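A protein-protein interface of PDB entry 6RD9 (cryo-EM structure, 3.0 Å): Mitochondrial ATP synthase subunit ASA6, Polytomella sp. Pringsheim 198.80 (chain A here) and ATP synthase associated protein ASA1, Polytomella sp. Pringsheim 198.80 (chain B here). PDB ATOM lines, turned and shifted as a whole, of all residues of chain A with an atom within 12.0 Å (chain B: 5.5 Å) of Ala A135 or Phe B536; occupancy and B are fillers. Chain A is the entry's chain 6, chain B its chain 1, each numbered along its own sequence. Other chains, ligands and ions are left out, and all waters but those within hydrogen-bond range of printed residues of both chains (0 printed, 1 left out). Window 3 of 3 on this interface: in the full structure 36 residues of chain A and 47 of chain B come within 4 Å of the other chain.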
ATOM      1  N   PRO A  60       7.677 -38.900 -31.041  1.00  0.00           N
ATOM      2  CA  PRO A  60       7.011 -37.788 -31.711  1.00  0.00           C
ATOM      3  C   PRO A  60       7.985 -37.006 -32.564  1.00  0.00           C
ATOM      4  O   PRO A  60       9.194 -37.016 -32.345  1.00  0.00           O
ATOM      5  CB  PRO A  60       6.491 -36.951 -30.553  1.00  0.00           C
ATOM      6  CG  PRO A  60       7.385 -37.246 -29.480  1.00  0.00           C
ATOM      7  CD  PRO A  60       7.754 -38.662 -29.595  1.00  0.00           C
ATOM      8  N   TYR A  62       9.918 -33.946 -33.634  1.00  0.00           N
ATOM      9  CA  TYR A  62      10.388 -32.636 -33.228  1.00  0.00           C
ATOM     10  C   TYR A  62      11.118 -32.101 -34.432  1.00  0.00           C
ATOM     11  O   TYR A  62      12.231 -32.576 -34.720  1.00  0.00           O
ATOM     12  CB  TYR A  62      11.316 -32.728 -32.031  1.00  0.00           C
ATOM     13  CG  TYR A  62      10.704 -33.383 -30.835  1.00  0.00           C
ATOM     14  CD1 TYR A  62       9.439 -33.066 -30.425  1.00  0.00           C
ATOM     15  CD2 TYR A  62      11.402 -34.319 -30.112  1.00  0.00           C
ATOM     16  CE1 TYR A  62       8.890 -33.657 -29.338  1.00  0.00           C
ATOM     17  CE2 TYR A  62      10.852 -34.912 -29.025  1.00  0.00           C
ATOM     18  CZ  TYR A  62       9.596 -34.571 -28.645  1.00  0.00           C
ATOM     19  OH  TYR A  62       9.047 -35.164 -27.552  1.00  0.00           O
ATOM     20  N   TYR A 126      10.809 -13.075 -15.920  1.00  0.00           N
ATOM     21  CA  TYR A 126      10.267 -14.186 -16.693  1.00  0.00           C
ATOM     22  C   TYR A 126       9.591 -15.197 -15.792  1.00  0.00           C
ATOM     23  O   TYR A 126       8.524 -15.713 -16.118  1.00  0.00           O
ATOM     24  CB  TYR A 126      11.374 -14.860 -17.488  1.00  0.00           C
ATOM     25  CG  TYR A 126      10.921 -16.078 -18.230  1.00  0.00           C
ATOM     26  CD1 TYR A 126      10.219 -15.963 -19.404  1.00  0.00           C
ATOM     27  CD2 TYR A 126      11.197 -17.344 -17.763  1.00  0.00           C
ATOM     28  CE1 TYR A 126       9.794 -17.060 -20.072  1.00  0.00           C
ATOM     29  CE2 TYR A 126      10.768 -18.441 -18.424  1.00  0.00           C
ATOM     30  CZ  TYR A 126      10.072 -18.289 -19.578  1.00  0.00           C
ATOM     31  OH  TYR A 126       9.646 -19.388 -20.250  1.00  0.00           O
ATOM     32  N   PHE A 127      10.193 -15.501 -14.660  1.00  0.00           N
ATOM     33  CA  PHE A 127       9.598 -16.461 -13.752  1.00  0.00           C
ATOM     34  C   PHE A 127       8.538 -15.842 -12.875  1.00  0.00           C
ATOM     35  O   PHE A 127       7.819 -16.576 -12.201  1.00  0.00           O
ATOM     36  CB  PHE A 127      10.674 -17.099 -12.888  1.00  0.00           C
ATOM     37  CG  PHE A 127      11.398 -18.201 -13.564  1.00  0.00           C
ATOM     38  CD1 PHE A 127      10.849 -19.449 -13.636  1.00  0.00           C
ATOM     39  CD2 PHE A 127      12.619 -17.986 -14.145  1.00  0.00           C
ATOM     40  CE1 PHE A 127      11.506 -20.453 -14.272  1.00  0.00           C
ATOM     41  CE2 PHE A 127      13.273 -18.986 -14.775  1.00  0.00           C
ATOM     42  CZ  PHE A 127      12.719 -20.216 -14.838  1.00  0.00           C
ATOM     43  N   ALA A 128       8.426 -14.525 -12.857  1.00  0.00           N
ATOM     44  CA  ALA A 128       7.323 -13.872 -12.179  1.00  0.00           C
ATOM     45  C   ALA A 128       6.091 -13.795 -13.042  1.00  0.00           C
ATOM     46  O   ALA A 128       4.989 -13.724 -12.509  1.00  0.00           O
ATOM     47  CB  ALA A 128       7.704 -12.464 -11.753  1.00  0.00           C
ATOM     48  N   PHE A 129       6.245 -13.764 -14.358  1.00  0.00           N
ATOM     49  CA  PHE A 129       5.078 -13.831 -15.222  1.00  0.00           C
ATOM     50  C   PHE A 129       4.586 -15.253 -15.343  1.00  0.00           C
ATOM     51  O   PHE A 129       3.401 -15.473 -15.571  1.00  0.00           O
ATOM     52  CB  PHE A 129       5.380 -13.272 -16.604  1.00  0.00           C
ATOM     53  CG  PHE A 129       5.526 -11.779 -16.643  1.00  0.00           C
ATOM     54  CD1 PHE A 129       5.205 -10.994 -15.566  1.00  0.00           C
ATOM     55  CD2 PHE A 129       5.990 -11.164 -17.766  1.00  0.00           C
ATOM     56  CE1 PHE A 129       5.351  -9.653 -15.617  1.00  0.00           C
ATOM     57  CE2 PHE A 129       6.124  -9.820 -17.818  1.00  0.00           C
ATOM     58  CZ  PHE A 129       5.807  -9.069 -16.744  1.00  0.00           C
ATOM     59  N   ARG A 130       5.469 -16.229 -15.168  1.00  0.00           N
ATOM     60  CA  ARG A 130       5.064 -17.624 -15.146  1.00  0.00           C
ATOM     61  C   ARG A 130       4.215 -17.961 -13.944  1.00  0.00           C
ATOM     62  O   ARG A 130       3.489 -18.948 -13.986  1.00  0.00           O
ATOM     63  CB  ARG A 130       6.278 -18.527 -15.150  1.00  0.00           C
ATOM     64  CG  ARG A 130       6.808 -18.777 -16.494  1.00  0.00           C
ATOM     65  CD  ARG A 130       7.897 -19.786 -16.456  1.00  0.00           C
ATOM     66  NE  ARG A 130       7.386 -21.129 -16.298  1.00  0.00           N
ATOM     67  CZ  ARG A 130       7.146 -21.945 -17.306  1.00  0.00           C
ATOM     68  NH1 ARG A 130       7.358 -21.552 -18.535  1.00  0.00           N
ATOM     69  NH2 ARG A 130       6.681 -23.152 -17.083  1.00  0.00           N
ATOM     70  N   GLY A 131       4.311 -17.201 -12.873  1.00  0.00           N
ATOM     71  CA  GLY A 131       3.442 -17.382 -11.739  1.00  0.00           C
ATOM     72  C   GLY A 131       2.143 -16.639 -11.809  1.00  0.00           C
ATOM     73  O   GLY A 131       1.267 -16.884 -10.989  1.00  0.00           O
ATOM     74  N   MET A 132       1.992 -15.724 -12.761  1.00  0.00           N
ATOM     75  CA  MET A 132       0.714 -15.052 -12.945  1.00  0.00           C
ATOM     76  C   MET A 132      -0.315 -15.993 -13.531  1.00  0.00           C
ATOM     77  O   MET A 132      -1.508 -15.872 -13.248  1.00  0.00           O
ATOM     78  CB  MET A 132       0.858 -13.852 -13.869  1.00  0.00           C
ATOM     79  CG  MET A 132       1.866 -12.855 -13.491  1.00  0.00           C
ATOM     80  SD  MET A 132       1.834 -11.505 -14.642  1.00  0.00           S
ATOM     81  CE  MET A 132       0.268 -10.800 -14.220  1.00  0.00           C
ATOM     82  N   ALA A 133       0.100 -16.854 -14.345  1.00  0.00           N
ATOM     83  CA  ALA A 133      -0.735 -17.830 -14.998  1.00  0.00           C
ATOM     84  C   ALA A 133      -0.777 -19.091 -14.174  1.00  0.00           C
ATOM     85  O   ALA A 133       0.274 -19.645 -13.873  1.00  0.00           O
ATOM     86  CB  ALA A 133      -0.189 -18.155 -16.362  1.00  0.00           C
ATOM     87  N   PRO A 134      -1.953 -19.594 -13.807  1.00  0.00           N
ATOM     88  CA  PRO A 134      -2.011 -20.871 -13.099  1.00  0.00           C
ATOM     89  C   PRO A 134      -1.592 -22.058 -13.933  1.00  0.00           C
ATOM     90  O   PRO A 134      -1.312 -23.108 -13.358  1.00  0.00           O
ATOM     91  CB  PRO A 134      -3.481 -20.975 -12.706  1.00  0.00           C
ATOM     92  CG  PRO A 134      -3.975 -19.652 -12.771  1.00  0.00           C
ATOM     93  CD  PRO A 134      -3.274 -18.974 -13.866  1.00  0.00           C
ATOM     94  N   ALA A 135      -1.534 -21.927 -15.255  1.00  0.00           N
ATOM     95  CA  ALA A 135      -1.088 -23.009 -16.115  1.00  0.00           C
ATOM     96  C   ALA A 135       0.400 -23.256 -16.002  1.00  0.00           C
ATOM     97  O   ALA A 135       0.863 -24.363 -16.274  1.00  0.00           O
ATOM     98  CB  ALA A 135      -1.434 -22.694 -17.554  1.00  0.00           C
ATOM     99  N   THR A 136       1.173 -22.250 -15.645  1.00  0.00           N
ATOM    100  CA  THR A 136       2.612 -22.387 -15.534  1.00  0.00           C
ATOM    101  C   THR A 136       3.095 -22.242 -14.107  1.00  0.00           C
ATOM    102  O   THR A 136       4.273 -22.448 -13.842  1.00  0.00           O
ATOM    103  CB  THR A 136       3.302 -21.353 -16.404  1.00  0.00           C
ATOM    104  OG1 THR A 136       2.875 -20.065 -15.990  1.00  0.00           O
ATOM    105  CG2 THR A 136       2.926 -21.508 -17.816  1.00  0.00           C
ATOM    106  N   ALA A 137       2.219 -21.884 -13.188  1.00  0.00           N
ATOM    107  CA  ALA A 137       2.570 -21.778 -11.790  1.00  0.00           C
ATOM    108  C   ALA A 137       2.697 -23.126 -11.105  1.00  0.00           C
ATOM    109  O   ALA A 137       3.188 -23.180  -9.976  1.00  0.00           O
ATOM    110  CB  ALA A 137       1.529 -20.935 -11.066  1.00  0.00           C
ATOM    111  N   SER A 138       2.277 -24.210 -11.747  1.00  0.00           N
ATOM    112  CA  SER A 138       2.328 -25.538 -11.167  1.00  0.00           C
ATOM    113  C   SER A 138       2.743 -26.505 -12.259  1.00  0.00           C
ATOM    114  O   SER A 138       3.115 -26.104 -13.360  1.00  0.00           O
ATOM    115  CB  SER A 138       0.972 -25.924 -10.578  1.00  0.00           C
ATOM    116  OG  SER A 138       0.593 -25.038  -9.558  1.00  0.00           O
ATOM    117  N   THR A 139       2.674 -27.790 -11.952  1.00  0.00           N
ATOM    118  CA  THR A 139       2.873 -28.857 -12.912  1.00  0.00           C
ATOM    119  C   THR A 139       1.504 -29.446 -13.211  1.00  0.00           C
ATOM    120  O   THR A 139       0.582 -29.293 -12.412  1.00  0.00           O
ATOM    121  CB  THR A 139       3.804 -29.915 -12.323  1.00  0.00           C
ATOM    122  OG1 THR A 139       4.876 -29.256 -11.656  1.00  0.00           O
ATOM    123  CG2 THR A 139       4.431 -30.778 -13.408  1.00  0.00           C
ATOM    124  N   LEU A 140       1.356 -30.096 -14.362  1.00  0.00           N
ATOM    125  CA  LEU A 140       0.129 -30.824 -14.633  1.00  0.00           C
ATOM    126  C   LEU A 140      -0.077 -31.956 -13.645  1.00  0.00           C
ATOM    127  O   LEU A 140       0.870 -32.528 -13.116  1.00  0.00           O
ATOM    128  CB  LEU A 140       0.123 -31.399 -16.029  1.00  0.00           C
ATOM    129  CG  LEU A 140      -0.481 -30.531 -17.085  1.00  0.00           C
ATOM    130  CD1 LEU A 140      -0.416 -31.334 -18.269  1.00  0.00           C
ATOM    131  CD2 LEU A 140      -1.891 -30.310 -16.739  1.00  0.00           C
ATOM    132  N   ASN A 141      -1.334 -32.300 -13.420  1.00  0.00           N
ATOM    133  CA  ASN A 141      -1.667 -33.043 -12.234  1.00  0.00           C
ATOM    134  C   ASN A 141      -2.415 -34.345 -12.442  1.00  0.00           C
ATOM    135  O   ASN A 141      -2.497 -35.123 -11.494  1.00  0.00           O
ATOM    136  CB  ASN A 141      -2.491 -32.179 -11.290  1.00  0.00           C
ATOM    137  CG  ASN A 141      -2.273 -32.538  -9.861  1.00  0.00           C
ATOM    138  OD1 ASN A 141      -1.234 -33.084  -9.512  1.00  0.00           O
ATOM    139  ND2 ASN A 141      -3.256 -32.253  -9.020  1.00  0.00           N
ATOM    140  N   GLY A 142      -2.961 -34.632 -13.602  1.00  0.00           N
ATOM    141  CA  GLY A 142      -3.725 -35.854 -13.729  1.00  0.00           C
ATOM    142  C   GLY A 142      -2.872 -37.084 -13.898  1.00  0.00           C
ATOM    143  O   GLY A 142      -1.653 -37.033 -13.804  1.00  0.00           O
ATOM    144  N   HIS B 531       3.185 -36.927 -22.817  1.00  0.00           N
ATOM    145  CA  HIS B 531       3.745 -35.971 -23.745  1.00  0.00           C
ATOM    146  C   HIS B 531       3.252 -34.570 -23.487  1.00  0.00           C
ATOM    147  O   HIS B 531       3.991 -33.620 -23.718  1.00  0.00           O
ATOM    148  CB  HIS B 531       3.413 -36.368 -25.164  1.00  0.00           C
ATOM    149  CG  HIS B 531       4.127 -35.556 -26.184  1.00  0.00           C
ATOM    150  ND1 HIS B 531       3.478 -34.692 -27.024  1.00  0.00           N
ATOM    151  CD2 HIS B 531       5.437 -35.448 -26.473  1.00  0.00           C
ATOM    152  CE1 HIS B 531       4.355 -34.105 -27.809  1.00  0.00           C
ATOM    153  NE2 HIS B 531       5.553 -34.550 -27.497  1.00  0.00           N
ATOM    154  N   ILE B 532       2.020 -34.414 -23.022  1.00  0.00           N
ATOM    155  CA  ILE B 532       1.564 -33.108 -22.583  1.00  0.00           C
ATOM    156  C   ILE B 532       2.352 -32.665 -21.370  1.00  0.00           C
ATOM    157  O   ILE B 532       2.927 -31.585 -21.372  1.00  0.00           O
ATOM    158  CB  ILE B 532       0.060 -33.126 -22.300  1.00  0.00           C
ATOM    159  CG1 ILE B 532      -0.695 -33.426 -23.567  1.00  0.00           C
ATOM    160  CG2 ILE B 532      -0.375 -31.816 -21.865  1.00  0.00           C
ATOM    161  CD1 ILE B 532      -2.148 -33.605 -23.371  1.00  0.00           C
ATOM    162  N   GLN B 533       2.466 -33.528 -20.362  1.00  0.00           N
ATOM    163  CA  GLN B 533       3.116 -33.162 -19.110  1.00  0.00           C
ATOM    164  C   GLN B 533       4.586 -32.835 -19.279  1.00  0.00           C
ATOM    165  O   GLN B 533       5.106 -31.948 -18.604  1.00  0.00           O
ATOM    166  CB  GLN B 533       2.962 -34.286 -18.110  1.00  0.00           C
ATOM    167  CG  GLN B 533       3.388 -33.910 -16.752  1.00  0.00           C
ATOM    168  CD  GLN B 533       3.285 -35.031 -15.820  1.00  0.00           C
ATOM    169  OE1 GLN B 533       3.811 -36.107 -16.070  1.00  0.00           O
ATOM    170  NE2 GLN B 533       2.587 -34.813 -14.725  1.00  0.00           N
ATOM    171  N   LYS B 534       5.251 -33.492 -20.212  1.00  0.00           N
ATOM    172  CA  LYS B 534       6.658 -33.239 -20.462  1.00  0.00           C
ATOM    173  C   LYS B 534       6.873 -31.888 -21.112  1.00  0.00           C
ATOM    174  O   LYS B 534       7.920 -31.274 -20.928  1.00  0.00           O
ATOM    175  CB  LYS B 534       7.187 -34.352 -21.348  1.00  0.00           C
ATOM    176  CG  LYS B 534       8.646 -34.399 -21.569  1.00  0.00           C
ATOM    177  CD  LYS B 534       8.951 -35.374 -22.647  1.00  0.00           C
ATOM    178  CE  LYS B 534      10.367 -35.225 -23.087  1.00  0.00           C
ATOM    179  NZ  LYS B 534      10.653 -36.097 -24.261  1.00  0.00           N
ATOM    180  N   HIS B 535       5.887 -31.401 -21.850  1.00  0.00           N
ATOM    181  CA  HIS B 535       6.046 -30.259 -22.722  1.00  0.00           C
ATOM    182  C   HIS B 535       5.106 -29.106 -22.441  1.00  0.00           C
ATOM    183  O   HIS B 535       5.294 -28.054 -23.038  1.00  0.00           O
ATOM    184  CB  HIS B 535       5.843 -30.681 -24.180  1.00  0.00           C
ATOM    185  CG  HIS B 535       6.982 -31.450 -24.756  1.00  0.00           C
ATOM    186  ND1 HIS B 535       8.198 -30.875 -25.031  1.00  0.00           N
ATOM    187  CD2 HIS B 535       7.085 -32.739 -25.134  1.00  0.00           C
ATOM    188  CE1 HIS B 535       9.009 -31.783 -25.531  1.00  0.00           C
ATOM    189  NE2 HIS B 535       8.357 -32.922 -25.606  1.00  0.00           N
ATOM    190  N   PHE B 536       4.096 -29.264 -21.597  1.00  0.00           N
ATOM    191  CA  PHE B 536       3.136 -28.193 -21.374  1.00  0.00           C
ATOM    192  C   PHE B 536       3.772 -27.082 -20.577  1.00  0.00           C
ATOM    193  O   PHE B 536       4.391 -27.329 -19.544  1.00  0.00           O
ATOM    194  CB  PHE B 536       1.923 -28.706 -20.621  1.00  0.00           C
ATOM    195  CG  PHE B 536       0.808 -27.750 -20.566  1.00  0.00           C
ATOM    196  CD1 PHE B 536       0.024 -27.535 -21.657  1.00  0.00           C
ATOM    197  CD2 PHE B 536       0.538 -27.067 -19.416  1.00  0.00           C
ATOM    198  CE1 PHE B 536      -0.983 -26.659 -21.602  1.00  0.00           C
ATOM    199  CE2 PHE B 536      -0.461 -26.199 -19.372  1.00  0.00           C
ATOM    200  CZ  PHE B 536      -1.226 -25.994 -20.462  1.00  0.00           C
ATOM    201  N   GLY B 537       3.605 -25.853 -21.042  1.00  0.00           N
ATOM    202  CA  GLY B 537       4.182 -24.724 -20.375  1.00  0.00           C
ATOM    203  C   GLY B 537       5.648 -24.542 -20.635  1.00  0.00           C
ATOM    204  O   GLY B 537       6.269 -23.681 -20.012  1.00  0.00           O
ATOM    205  N   ILE B 538       6.229 -25.335 -21.520  1.00  0.00           N
ATOM    206  CA  ILE B 538       7.618 -25.182 -21.902  1.00  0.00           C
ATOM    207  C   ILE B 538       7.671 -24.954 -23.398  1.00  0.00           C
ATOM    208  O   ILE B 538       7.999 -23.858 -23.844  1.00  0.00           O
ATOM    209  CB  ILE B 538       8.454 -26.402 -21.491  1.00  0.00           C
ATOM    210  CG1 ILE B 538       8.530 -26.509 -19.986  1.00  0.00           C
ATOM    211  CG2 ILE B 538       9.825 -26.278 -21.991  1.00  0.00           C
ATOM    212  CD1 ILE B 538       8.834 -27.853 -19.520  1.00  0.00           C
ATOM    213  N   ASP B 539       7.324 -25.953 -24.192  1.00  0.00           N
ATOM    214  CA  ASP B 539       7.393 -25.746 -25.628  1.00  0.00           C
ATOM    215  C   ASP B 539       6.296 -26.425 -26.425  1.00  0.00           C
ATOM    216  O   ASP B 539       6.457 -26.554 -27.633  1.00  0.00           O
ATOM    217  CB  ASP B 539       8.745 -26.182 -26.199  1.00  0.00           C
ATOM    218  CG  ASP B 539       9.225 -27.521 -25.669  1.00  0.00           C
ATOM    219  OD1 ASP B 539       8.412 -28.406 -25.393  1.00  0.00           O
ATOM    220  OD2 ASP B 539      10.445 -27.703 -25.534  1.00  0.00           O
ATOM    221  N   LEU B 540       5.224 -26.878 -25.823  1.00  0.00           N
ATOM    222  CA  LEU B 540       4.232 -27.625 -26.579  1.00  0.00           C
ATOM    223  C   LEU B 540       3.433 -26.663 -27.431  1.00  0.00           C
ATOM    224  O   LEU B 540       2.964 -25.660 -26.918  1.00  0.00           O
ATOM    225  CB  LEU B 540       3.305 -28.366 -25.639  1.00  0.00           C
ATOM    226  CG  LEU B 540       2.255 -29.389 -26.045  1.00  0.00           C
ATOM    227  CD1 LEU B 540       2.845 -30.531 -26.721  1.00  0.00           C
ATOM    228  CD2 LEU B 540       1.622 -29.836 -24.824  1.00  0.00           C
ATOM    229  N   VAL B 545      -1.624 -30.066 -28.969  1.00  0.00           N
ATOM    230  CA  VAL B 545      -2.666 -30.288 -27.976  1.00  0.00           C
ATOM    231  C   VAL B 545      -3.992 -30.567 -28.654  1.00  0.00           C
ATOM    232  O   VAL B 545      -4.700 -31.510 -28.309  1.00  0.00           O
ATOM    233  CB  VAL B 545      -2.776 -29.070 -27.058  1.00  0.00           C
ATOM    234  CG1 VAL B 545      -3.933 -29.209 -26.189  1.00  0.00           C
ATOM    235  CG2 VAL B 545      -1.577 -28.925 -26.265  1.00  0.00           C
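The side-chain hydroxyl (OH) of Tyr A62 is in hydrogen-bond range of a ring nitrogen (NE2) of His B535 (3.0 Å).
O of Leu A140 sits at hydrogen-bond distance from NE2 of Gln B533, at 3.3 Å.
O of Gly B537 is in hydrogen-bond range of NH1 of Arg A130, at 2.8 Å.
The backbone carbonyl oxygen (O) of His B535 lies within hydrogen-bond range of the backbone NH (N) of Leu B540 (3.0 Å).
O of Arg A130 is in hydrogen-bond range of N of Ala A137.
A ring nitrogen (ND1) of His B535 is in hydrogen-bond range of the side-chain carboxylate of Asp B539 (2.5 Å).
Among the printed residues, pairs that only touch across the chains: Pro A60 with His B531, Tyr A62 with His B531, Tyr A62 with Lys B534, Ala A135 with Phe B536 and Leu A140 with Ile B532.
Of chain B, only Phe B536 (3.8 Å) comes within 4 Å of Ala A135.
Printed residues of chain A within 4 Å of Phe B536: Ala A135.
No residue of chain A comes within 4 Å of Asp B539.
Of the printed residues of chain A, Lys B534 touches Tyr A62 (3.8 Å).
Of the printed residues of chain A, His B531 touches Pro A60 and Tyr A62.
Printed residues of chain B within 4 Å of Arg A130: Gly B537 (2.8 Å).
Of the printed residues of chain B, Leu A140 touches Ile B532 and Gln B533.
Of the printed residues of chain B, Pro A60 touches His B531.
Ala A128 touches none of the printed residues of chain B.
Tyr A126 touches none of the printed residues of chain B.
The nearest residue of chain B that does not touch Ala A135 is Gly B537 (5.3 Å).
The nearest printed residue of chain A that does not touch Gln B533 is Thr A139 (4.6 Å).
Printed residues of chain B that touch a printed residue of chain A: His B531, Ile B532, Gln B533, Lys B534, His B535, Phe B536 and Gly B537.
Hydrophobic or aromatic side chains of chain B that line the printed part of chain A: His B531, Ile B532, His B535 and Phe B536.
Among the printed residues, 8 pairs touch across the chains.
Among the printed residues, no Asp or Glu carboxylate lies within 4 Å of a Lys or Arg side-chain nitrogen of the other chain.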
